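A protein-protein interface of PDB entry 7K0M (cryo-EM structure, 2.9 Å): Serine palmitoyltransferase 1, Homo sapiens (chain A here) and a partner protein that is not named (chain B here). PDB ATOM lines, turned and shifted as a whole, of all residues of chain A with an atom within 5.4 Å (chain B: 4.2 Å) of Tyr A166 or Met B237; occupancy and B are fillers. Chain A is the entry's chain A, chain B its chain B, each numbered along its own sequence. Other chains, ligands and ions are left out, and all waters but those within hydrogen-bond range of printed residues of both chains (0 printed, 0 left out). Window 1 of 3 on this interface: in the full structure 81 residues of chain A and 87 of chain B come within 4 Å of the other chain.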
ATOM      1  N   TYR A 164      -5.664 -22.870  13.199  1.00  0.00           N
ATOM      2  CA  TYR A 164      -4.325 -22.326  13.335  1.00  0.00           C
ATOM      3  C   TYR A 164      -4.034 -22.095  14.809  1.00  0.00           C
ATOM      4  O   TYR A 164      -4.944 -21.919  15.624  1.00  0.00           O
ATOM      5  CB  TYR A 164      -4.174 -21.010  12.568  1.00  0.00           C
ATOM      6  CG  TYR A 164      -4.269 -21.133  11.069  1.00  0.00           C
ATOM      7  CD1 TYR A 164      -5.493 -21.304  10.442  1.00  0.00           C
ATOM      8  CD2 TYR A 164      -3.136 -21.053  10.278  1.00  0.00           C
ATOM      9  CE1 TYR A 164      -5.582 -21.404   9.075  1.00  0.00           C
ATOM     10  CE2 TYR A 164      -3.217 -21.153   8.910  1.00  0.00           C
ATOM     11  CZ  TYR A 164      -4.441 -21.329   8.314  1.00  0.00           C
ATOM     12  OH  TYR A 164      -4.524 -21.429   6.949  1.00  0.00           O
ATOM     13  N   SER A 165      -2.748 -22.080  15.147  1.00  0.00           N
ATOM     14  CA  SER A 165      -2.311 -21.915  16.524  1.00  0.00           C
ATOM     15  C   SER A 165      -2.076 -20.460  16.902  1.00  0.00           C
ATOM     16  O   SER A 165      -1.417 -20.195  17.913  1.00  0.00           O
ATOM     17  CB  SER A 165      -1.039 -22.722  16.773  1.00  0.00           C
ATOM     18  OG  SER A 165      -0.084 -22.487  15.756  1.00  0.00           O
ATOM     19  N   TYR A 166      -2.604 -19.510  16.129  1.00  0.00           N
ATOM     20  CA  TYR A 166      -2.307 -18.112  16.402  1.00  0.00           C
ATOM     21  C   TYR A 166      -3.319 -17.243  15.663  1.00  0.00           C
ATOM     22  O   TYR A 166      -3.597 -17.485  14.486  1.00  0.00           O
ATOM     23  CB  TYR A 166      -0.881 -17.805  15.958  1.00  0.00           C
ATOM     24  CG  TYR A 166      -0.265 -16.556  16.530  1.00  0.00           C
ATOM     25  CD1 TYR A 166      -0.270 -16.335  17.896  1.00  0.00           C
ATOM     26  CD2 TYR A 166       0.410 -15.654  15.725  1.00  0.00           C
ATOM     27  CE1 TYR A 166       0.322 -15.226  18.437  1.00  0.00           C
ATOM     28  CE2 TYR A 166       1.001 -14.536  16.261  1.00  0.00           C
ATOM     29  CZ  TYR A 166       0.958 -14.331  17.618  1.00  0.00           C
ATOM     30  OH  TYR A 166       1.554 -13.223  18.161  1.00  0.00           O
ATOM     31  N   GLY A 167      -3.888 -16.246  16.341  1.00  0.00           N
ATOM     32  CA  GLY A 167      -5.002 -15.511  15.758  1.00  0.00           C
ATOM     33  C   GLY A 167      -4.627 -14.712  14.524  1.00  0.00           C
ATOM     34  O   GLY A 167      -5.357 -14.710  13.530  1.00  0.00           O
ATOM     35  N   PHE A 168      -3.495 -14.009  14.576  1.00  0.00           N
ATOM     36  CA  PHE A 168      -3.050 -13.201  13.444  1.00  0.00           C
ATOM     37  C   PHE A 168      -2.810 -14.071  12.212  1.00  0.00           C
ATOM     38  O   PHE A 168      -3.308 -13.781  11.110  1.00  0.00           O
ATOM     39  CB  PHE A 168      -1.772 -12.464  13.845  1.00  0.00           C
ATOM     40  CG  PHE A 168      -1.546 -11.166  13.126  1.00  0.00           C
ATOM     41  CD1 PHE A 168      -1.057 -11.146  11.833  1.00  0.00           C
ATOM     42  CD2 PHE A 168      -1.776  -9.964  13.767  1.00  0.00           C
ATOM     43  CE1 PHE A 168      -0.828  -9.952  11.187  1.00  0.00           C
ATOM     44  CE2 PHE A 168      -1.550  -8.769  13.124  1.00  0.00           C
ATOM     45  CZ  PHE A 168      -1.075  -8.762  11.834  1.00  0.00           C
ATOM     46  N   ALA A 169      -2.073 -15.169  12.402  1.00  0.00           N
ATOM     47  CA  ALA A 169      -1.662 -16.013  11.290  1.00  0.00           C
ATOM     48  C   ALA A 169      -2.852 -16.626  10.574  1.00  0.00           C
ATOM     49  O   ALA A 169      -2.758 -16.921   9.382  1.00  0.00           O
ATOM     50  CB  ALA A 169      -0.722 -17.110  11.786  1.00  0.00           C
ATOM     51  N   THR A 170      -3.983 -16.782  11.260  1.00  0.00           N
ATOM     52  CA  THR A 170      -5.160 -17.388  10.650  1.00  0.00           C
ATOM     53  C   THR A 170      -5.545 -16.668   9.368  1.00  0.00           C
ATOM     54  O   THR A 170      -5.436 -17.233   8.277  1.00  0.00           O
ATOM     55  CB  THR A 170      -6.337 -17.373  11.623  1.00  0.00           C
ATOM     56  OG1 THR A 170      -6.003 -18.125  12.794  1.00  0.00           O
ATOM     57  CG2 THR A 170      -7.562 -17.978  10.974  1.00  0.00           C
ATOM     58  N   GLU A 308      -9.580 -16.340  20.701  1.00  0.00           N
ATOM     59  CA  GLU A 308      -9.037 -15.620  21.847  1.00  0.00           C
ATOM     60  C   GLU A 308     -10.037 -14.661  22.481  1.00  0.00           C
ATOM     61  O   GLU A 308     -10.091 -14.554  23.710  1.00  0.00           O
ATOM     62  CB  GLU A 308      -7.781 -14.856  21.425  1.00  0.00           C
ATOM     63  CG  GLU A 308      -6.680 -15.749  20.876  1.00  0.00           C
ATOM     64  CD  GLU A 308      -5.779 -15.037  19.893  1.00  0.00           C
ATOM     65  OE1 GLU A 308      -6.117 -13.908  19.485  1.00  0.00           O
ATOM     66  OE2 GLU A 308      -4.729 -15.607  19.527  1.00  0.00           O
ATOM     67  N   ILE A 314      -5.807 -19.499  23.151  1.00  0.00           N
ATOM     68  CA  ILE A 314      -4.987 -19.131  22.003  1.00  0.00           C
ATOM     69  C   ILE A 314      -5.422 -19.931  20.784  1.00  0.00           C
ATOM     70  O   ILE A 314      -5.862 -21.080  20.891  1.00  0.00           O
ATOM     71  CB  ILE A 314      -3.496 -19.347  22.322  1.00  0.00           C
ATOM     72  CG1 ILE A 314      -3.195 -18.916  23.756  1.00  0.00           C
ATOM     73  CG2 ILE A 314      -2.625 -18.573  21.352  1.00  0.00           C
ATOM     74  CD1 ILE A 314      -3.335 -17.430  23.987  1.00  0.00           C
ATOM     75  N   GLY A 315      -5.314 -19.318  19.613  1.00  0.00           N
ATOM     76  CA  GLY A 315      -5.574 -19.984  18.355  1.00  0.00           C
ATOM     77  C   GLY A 315      -6.496 -19.182  17.458  1.00  0.00           C
ATOM     78  O   GLY A 315      -6.887 -18.056  17.760  1.00  0.00           O
ATOM     79  N   GLY A 316      -6.832 -19.796  16.323  1.00  0.00           N
ATOM     80  CA  GLY A 316      -7.782 -19.229  15.386  1.00  0.00           C
ATOM     81  C   GLY A 316      -8.306 -20.330  14.493  1.00  0.00           C
ATOM     82  O   GLY A 316      -7.792 -21.447  14.499  1.00  0.00           O
ATOM     83  N   GLY A 334       1.098 -20.514   7.673  1.00  0.00           N
ATOM     84  CA  GLY A 334       1.056 -20.618   9.119  1.00  0.00           C
ATOM     85  C   GLY A 334       0.625 -21.979   9.618  1.00  0.00           C
ATOM     86  O   GLY A 334       0.792 -22.276  10.804  1.00  0.00           O
ATOM     87  N   SER A 338       4.526 -24.615  10.881  1.00  0.00           N
ATOM     88  CA  SER A 338       4.473 -24.186  12.268  1.00  0.00           C
ATOM     89  C   SER A 338       3.934 -25.312  13.134  1.00  0.00           C
ATOM     90  O   SER A 338       3.211 -26.189  12.658  1.00  0.00           O
ATOM     91  CB  SER A 338       3.608 -22.937  12.436  1.00  0.00           C
ATOM     92  OG  SER A 338       3.575 -22.531  13.791  1.00  0.00           O
ATOM     93  N   TYR B 235       7.500 -14.049  22.274  1.00  0.00           N
ATOM     94  CA  TYR B 235       6.292 -14.039  21.465  1.00  0.00           C
ATOM     95  C   TYR B 235       5.640 -15.412  21.510  1.00  0.00           C
ATOM     96  O   TYR B 235       6.246 -16.398  21.936  1.00  0.00           O
ATOM     97  CB  TYR B 235       6.584 -13.654  20.012  1.00  0.00           C
ATOM     98  CG  TYR B 235       7.513 -12.478  19.860  1.00  0.00           C
ATOM     99  CD1 TYR B 235       7.023 -11.184  19.826  1.00  0.00           C
ATOM    100  CD2 TYR B 235       8.879 -12.662  19.743  1.00  0.00           C
ATOM    101  CE1 TYR B 235       7.866 -10.108  19.683  1.00  0.00           C
ATOM    102  CE2 TYR B 235       9.732 -11.591  19.603  1.00  0.00           C
ATOM    103  CZ  TYR B 235       9.220 -10.317  19.572  1.00  0.00           C
ATOM    104  OH  TYR B 235      10.066  -9.245  19.431  1.00  0.00           O
ATOM    105  N   GLY B 236       4.396 -15.468  21.046  1.00  0.00           N
ATOM    106  CA  GLY B 236       3.575 -16.656  21.127  1.00  0.00           C
ATOM    107  C   GLY B 236       3.650 -17.614  19.959  1.00  0.00           C
ATOM    108  O   GLY B 236       2.855 -18.557  19.909  1.00  0.00           O
ATOM    109  N   MET B 237       4.570 -17.413  19.018  1.00  0.00           N
ATOM    110  CA  MET B 237       4.677 -18.299  17.869  1.00  0.00           C
ATOM    111  C   MET B 237       6.044 -18.104  17.229  1.00  0.00           C
ATOM    112  O   MET B 237       6.497 -16.971  17.064  1.00  0.00           O
ATOM    113  CB  MET B 237       3.565 -18.015  16.856  1.00  0.00           C
ATOM    114  CG  MET B 237       3.529 -18.935  15.653  1.00  0.00           C
ATOM    115  SD  MET B 237       2.118 -18.525  14.616  1.00  0.00           S
ATOM    116  CE  MET B 237       2.321 -19.636  13.237  1.00  0.00           C
ATOM    117  N   GLY B 238       6.697 -19.214  16.881  1.00  0.00           N
ATOM    118  CA  GLY B 238       8.003 -19.124  16.248  1.00  0.00           C
ATOM    119  C   GLY B 238       7.945 -18.548  14.847  1.00  0.00           C
ATOM    120  O   GLY B 238       8.805 -17.755  14.456  1.00  0.00           O
ATOM    121  N   PHE B 239       6.945 -18.953  14.066  1.00  0.00           N
ATOM    122  CA  PHE B 239       6.740 -18.384  12.739  1.00  0.00           C
ATOM    123  C   PHE B 239       6.472 -16.886  12.823  1.00  0.00           C
ATOM    124  O   PHE B 239       7.051 -16.090  12.067  1.00  0.00           O
ATOM    125  CB  PHE B 239       5.573 -19.112  12.070  1.00  0.00           C
ATOM    126  CG  PHE B 239       5.473 -18.904  10.590  1.00  0.00           C
ATOM    127  CD1 PHE B 239       4.752 -17.846  10.076  1.00  0.00           C
ATOM    128  CD2 PHE B 239       6.063 -19.790   9.712  1.00  0.00           C
ATOM    129  CE1 PHE B 239       4.647 -17.660   8.719  1.00  0.00           C
ATOM    130  CE2 PHE B 239       5.959 -19.607   8.353  1.00  0.00           C
ATOM    131  CZ  PHE B 239       5.251 -18.540   7.857  1.00  0.00           C
ATOM    132  N   ALA B 240       5.610 -16.485  13.760  1.00  0.00           N
ATOM    133  CA  ALA B 240       5.238 -15.086  13.899  1.00  0.00           C
ATOM    134  C   ALA B 240       6.416 -14.221  14.307  1.00  0.00           C
ATOM    135  O   ALA B 240       6.481 -13.056  13.910  1.00  0.00           O
ATOM    136  CB  ALA B 240       4.111 -14.942  14.915  1.00  0.00           C
ATOM    137  N   THR B 241       7.349 -14.761  15.091  1.00  0.00           N
ATOM    138  CA  THR B 241       8.531 -13.997  15.477  1.00  0.00           C
ATOM    139  C   THR B 241       9.234 -13.428  14.251  1.00  0.00           C
ATOM    140  O   THR B 241       9.378 -12.209  14.110  1.00  0.00           O
ATOM    141  CB  THR B 241       9.484 -14.877  16.284  1.00  0.00           C
ATOM    142  OG1 THR B 241       8.782 -15.458  17.387  1.00  0.00           O
ATOM    143  CG2 THR B 241      10.626 -14.050  16.812  1.00  0.00           C
ATOM    144  N   MET B 244       6.945 -11.144  11.839  1.00  0.00           N
ATOM    145  CA  MET B 244       6.472  -9.895  12.396  1.00  0.00           C
ATOM    146  C   MET B 244       7.591  -9.016  12.922  1.00  0.00           C
ATOM    147  O   MET B 244       7.337  -7.852  13.246  1.00  0.00           O
ATOM    148  CB  MET B 244       5.485 -10.191  13.528  1.00  0.00           C
ATOM    149  CG  MET B 244       4.211 -10.835  13.040  1.00  0.00           C
ATOM    150  SD  MET B 244       3.070 -11.188  14.376  1.00  0.00           S
ATOM    151  CE  MET B 244       1.779 -12.010  13.474  1.00  0.00           C
ATOM    152  N   GLY B 385       6.144 -21.117  21.510  1.00  0.00           N
ATOM    153  CA  GLY B 385       6.569 -19.751  21.707  1.00  0.00           C
ATOM    154  C   GLY B 385       7.810 -19.450  20.900  1.00  0.00           C
ATOM    155  O   GLY B 385       8.272 -20.263  20.105  1.00  0.00           O
ATOM    156  N   SER B 404       3.485  -8.040  16.449  1.00  0.00           N
ATOM    157  CA  SER B 404       2.902  -8.905  17.467  1.00  0.00           C
ATOM    158  C   SER B 404       2.809  -8.210  18.816  1.00  0.00           C
ATOM    159  O   SER B 404       2.030  -8.633  19.676  1.00  0.00           O
ATOM    160  CB  SER B 404       3.719 -10.188  17.595  1.00  0.00           C
ATOM    161  OG  SER B 404       5.082  -9.894  17.825  1.00  0.00           O
ATOM    162  N   ALA B 408      -1.256  -8.559  18.390  1.00  0.00           N
ATOM    163  CA  ALA B 408      -1.385  -9.992  18.600  1.00  0.00           C
ATOM    164  C   ALA B 408      -1.436 -10.329  20.083  1.00  0.00           C
ATOM    165  O   ALA B 408      -0.768  -9.691  20.900  1.00  0.00           O
ATOM    166  CB  ALA B 408      -0.235 -10.739  17.940  1.00  0.00           C
ATOM    167  N   THR B 409      -2.228 -11.345  20.416  1.00  0.00           N
ATOM    168  CA  THR B 409      -2.348 -11.804  21.792  1.00  0.00           C
ATOM    169  C   THR B 409      -1.039 -12.428  22.266  1.00  0.00           C
ATOM    170  O   THR B 409      -0.362 -13.135  21.515  1.00  0.00           O
ATOM    171  CB  THR B 409      -3.492 -12.813  21.904  1.00  0.00           C
ATOM    172  OG1 THR B 409      -4.732 -12.160  21.608  1.00  0.00           O
ATOM    173  CG2 THR B 409      -3.566 -13.404  23.293  1.00  0.00           C
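The side-chain hydroxyl (OG1) of Thr B241 sits at hydrogen-bond distance from the backbone carbonyl oxygen (O) of Met B237. The side-chain hydroxyl (OG1) of Thr A170 sits at hydrogen-bond distance from the backbone carbonyl oxygen (O) of Tyr A166. The side-chain sulfur (SD) of Met B244 sits close to the backbone NH (N) of Ser B404 (3.8 Å). The backbone NH (N) of Gly A167 sits at hydrogen-bond distance from the side-chain carboxylate (OE2) of Glu A308 (3.4 Å).
Among the printed residues, merely in contact across the chains: Tyr A166 with Met B237 (3.4 Å), Tyr A166 with Ala B240 (3.4 Å), Tyr A166 with Met B244 (3.8 Å), Tyr A166 with Ser B404 (3.8 Å), Tyr A166 with Ala B408 (3.1 Å), Tyr A166 with Thr B409 (3.8 Å), Phe A168 with Met B244 (3.4 Å), Gly A334 with Met B237 (3.9 Å) and Ser A338 with Met B237 (3.2 Å).
Tyr A166 touches just these residues of chain B: Met B237, Ala B240, Met B244, Ser B404, Ala B408 and Thr B409. Of the printed residues of chain B, Ser A338 touches Met B237. Met B237 touches just these residues of chain A: Tyr A166 (3.4 Å), Gly A334 (3.9 Å) and Ser A338 (3.2 Å). Of the printed residues of chain A, Ala B240 touches Tyr A166. Of the printed residues of chain A, Ala B408 touches Tyr A166.
The side-chain carboxylate (OE1) of Glu A308 lies within hydrogen-bond range of the side-chain hydroxyl (OG1) of Thr B409, at 3.1 Å.
Of the 13 printed residues of chain A, 5 touch a printed residue of chain B. Of the 12 printed residues of chain B, 6 touch a printed residue of chain A. Printed residues of chain B that touch a printed residue of chain A: Met B237, Ala B240, Met B244, Ser B404, Ala B408 and Thr B409. Hydrophobic or aromatic side chains of chain B within 4 Å of the printed part of chain A: Met B237, Ala B240, Met B244 and Ala B408.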
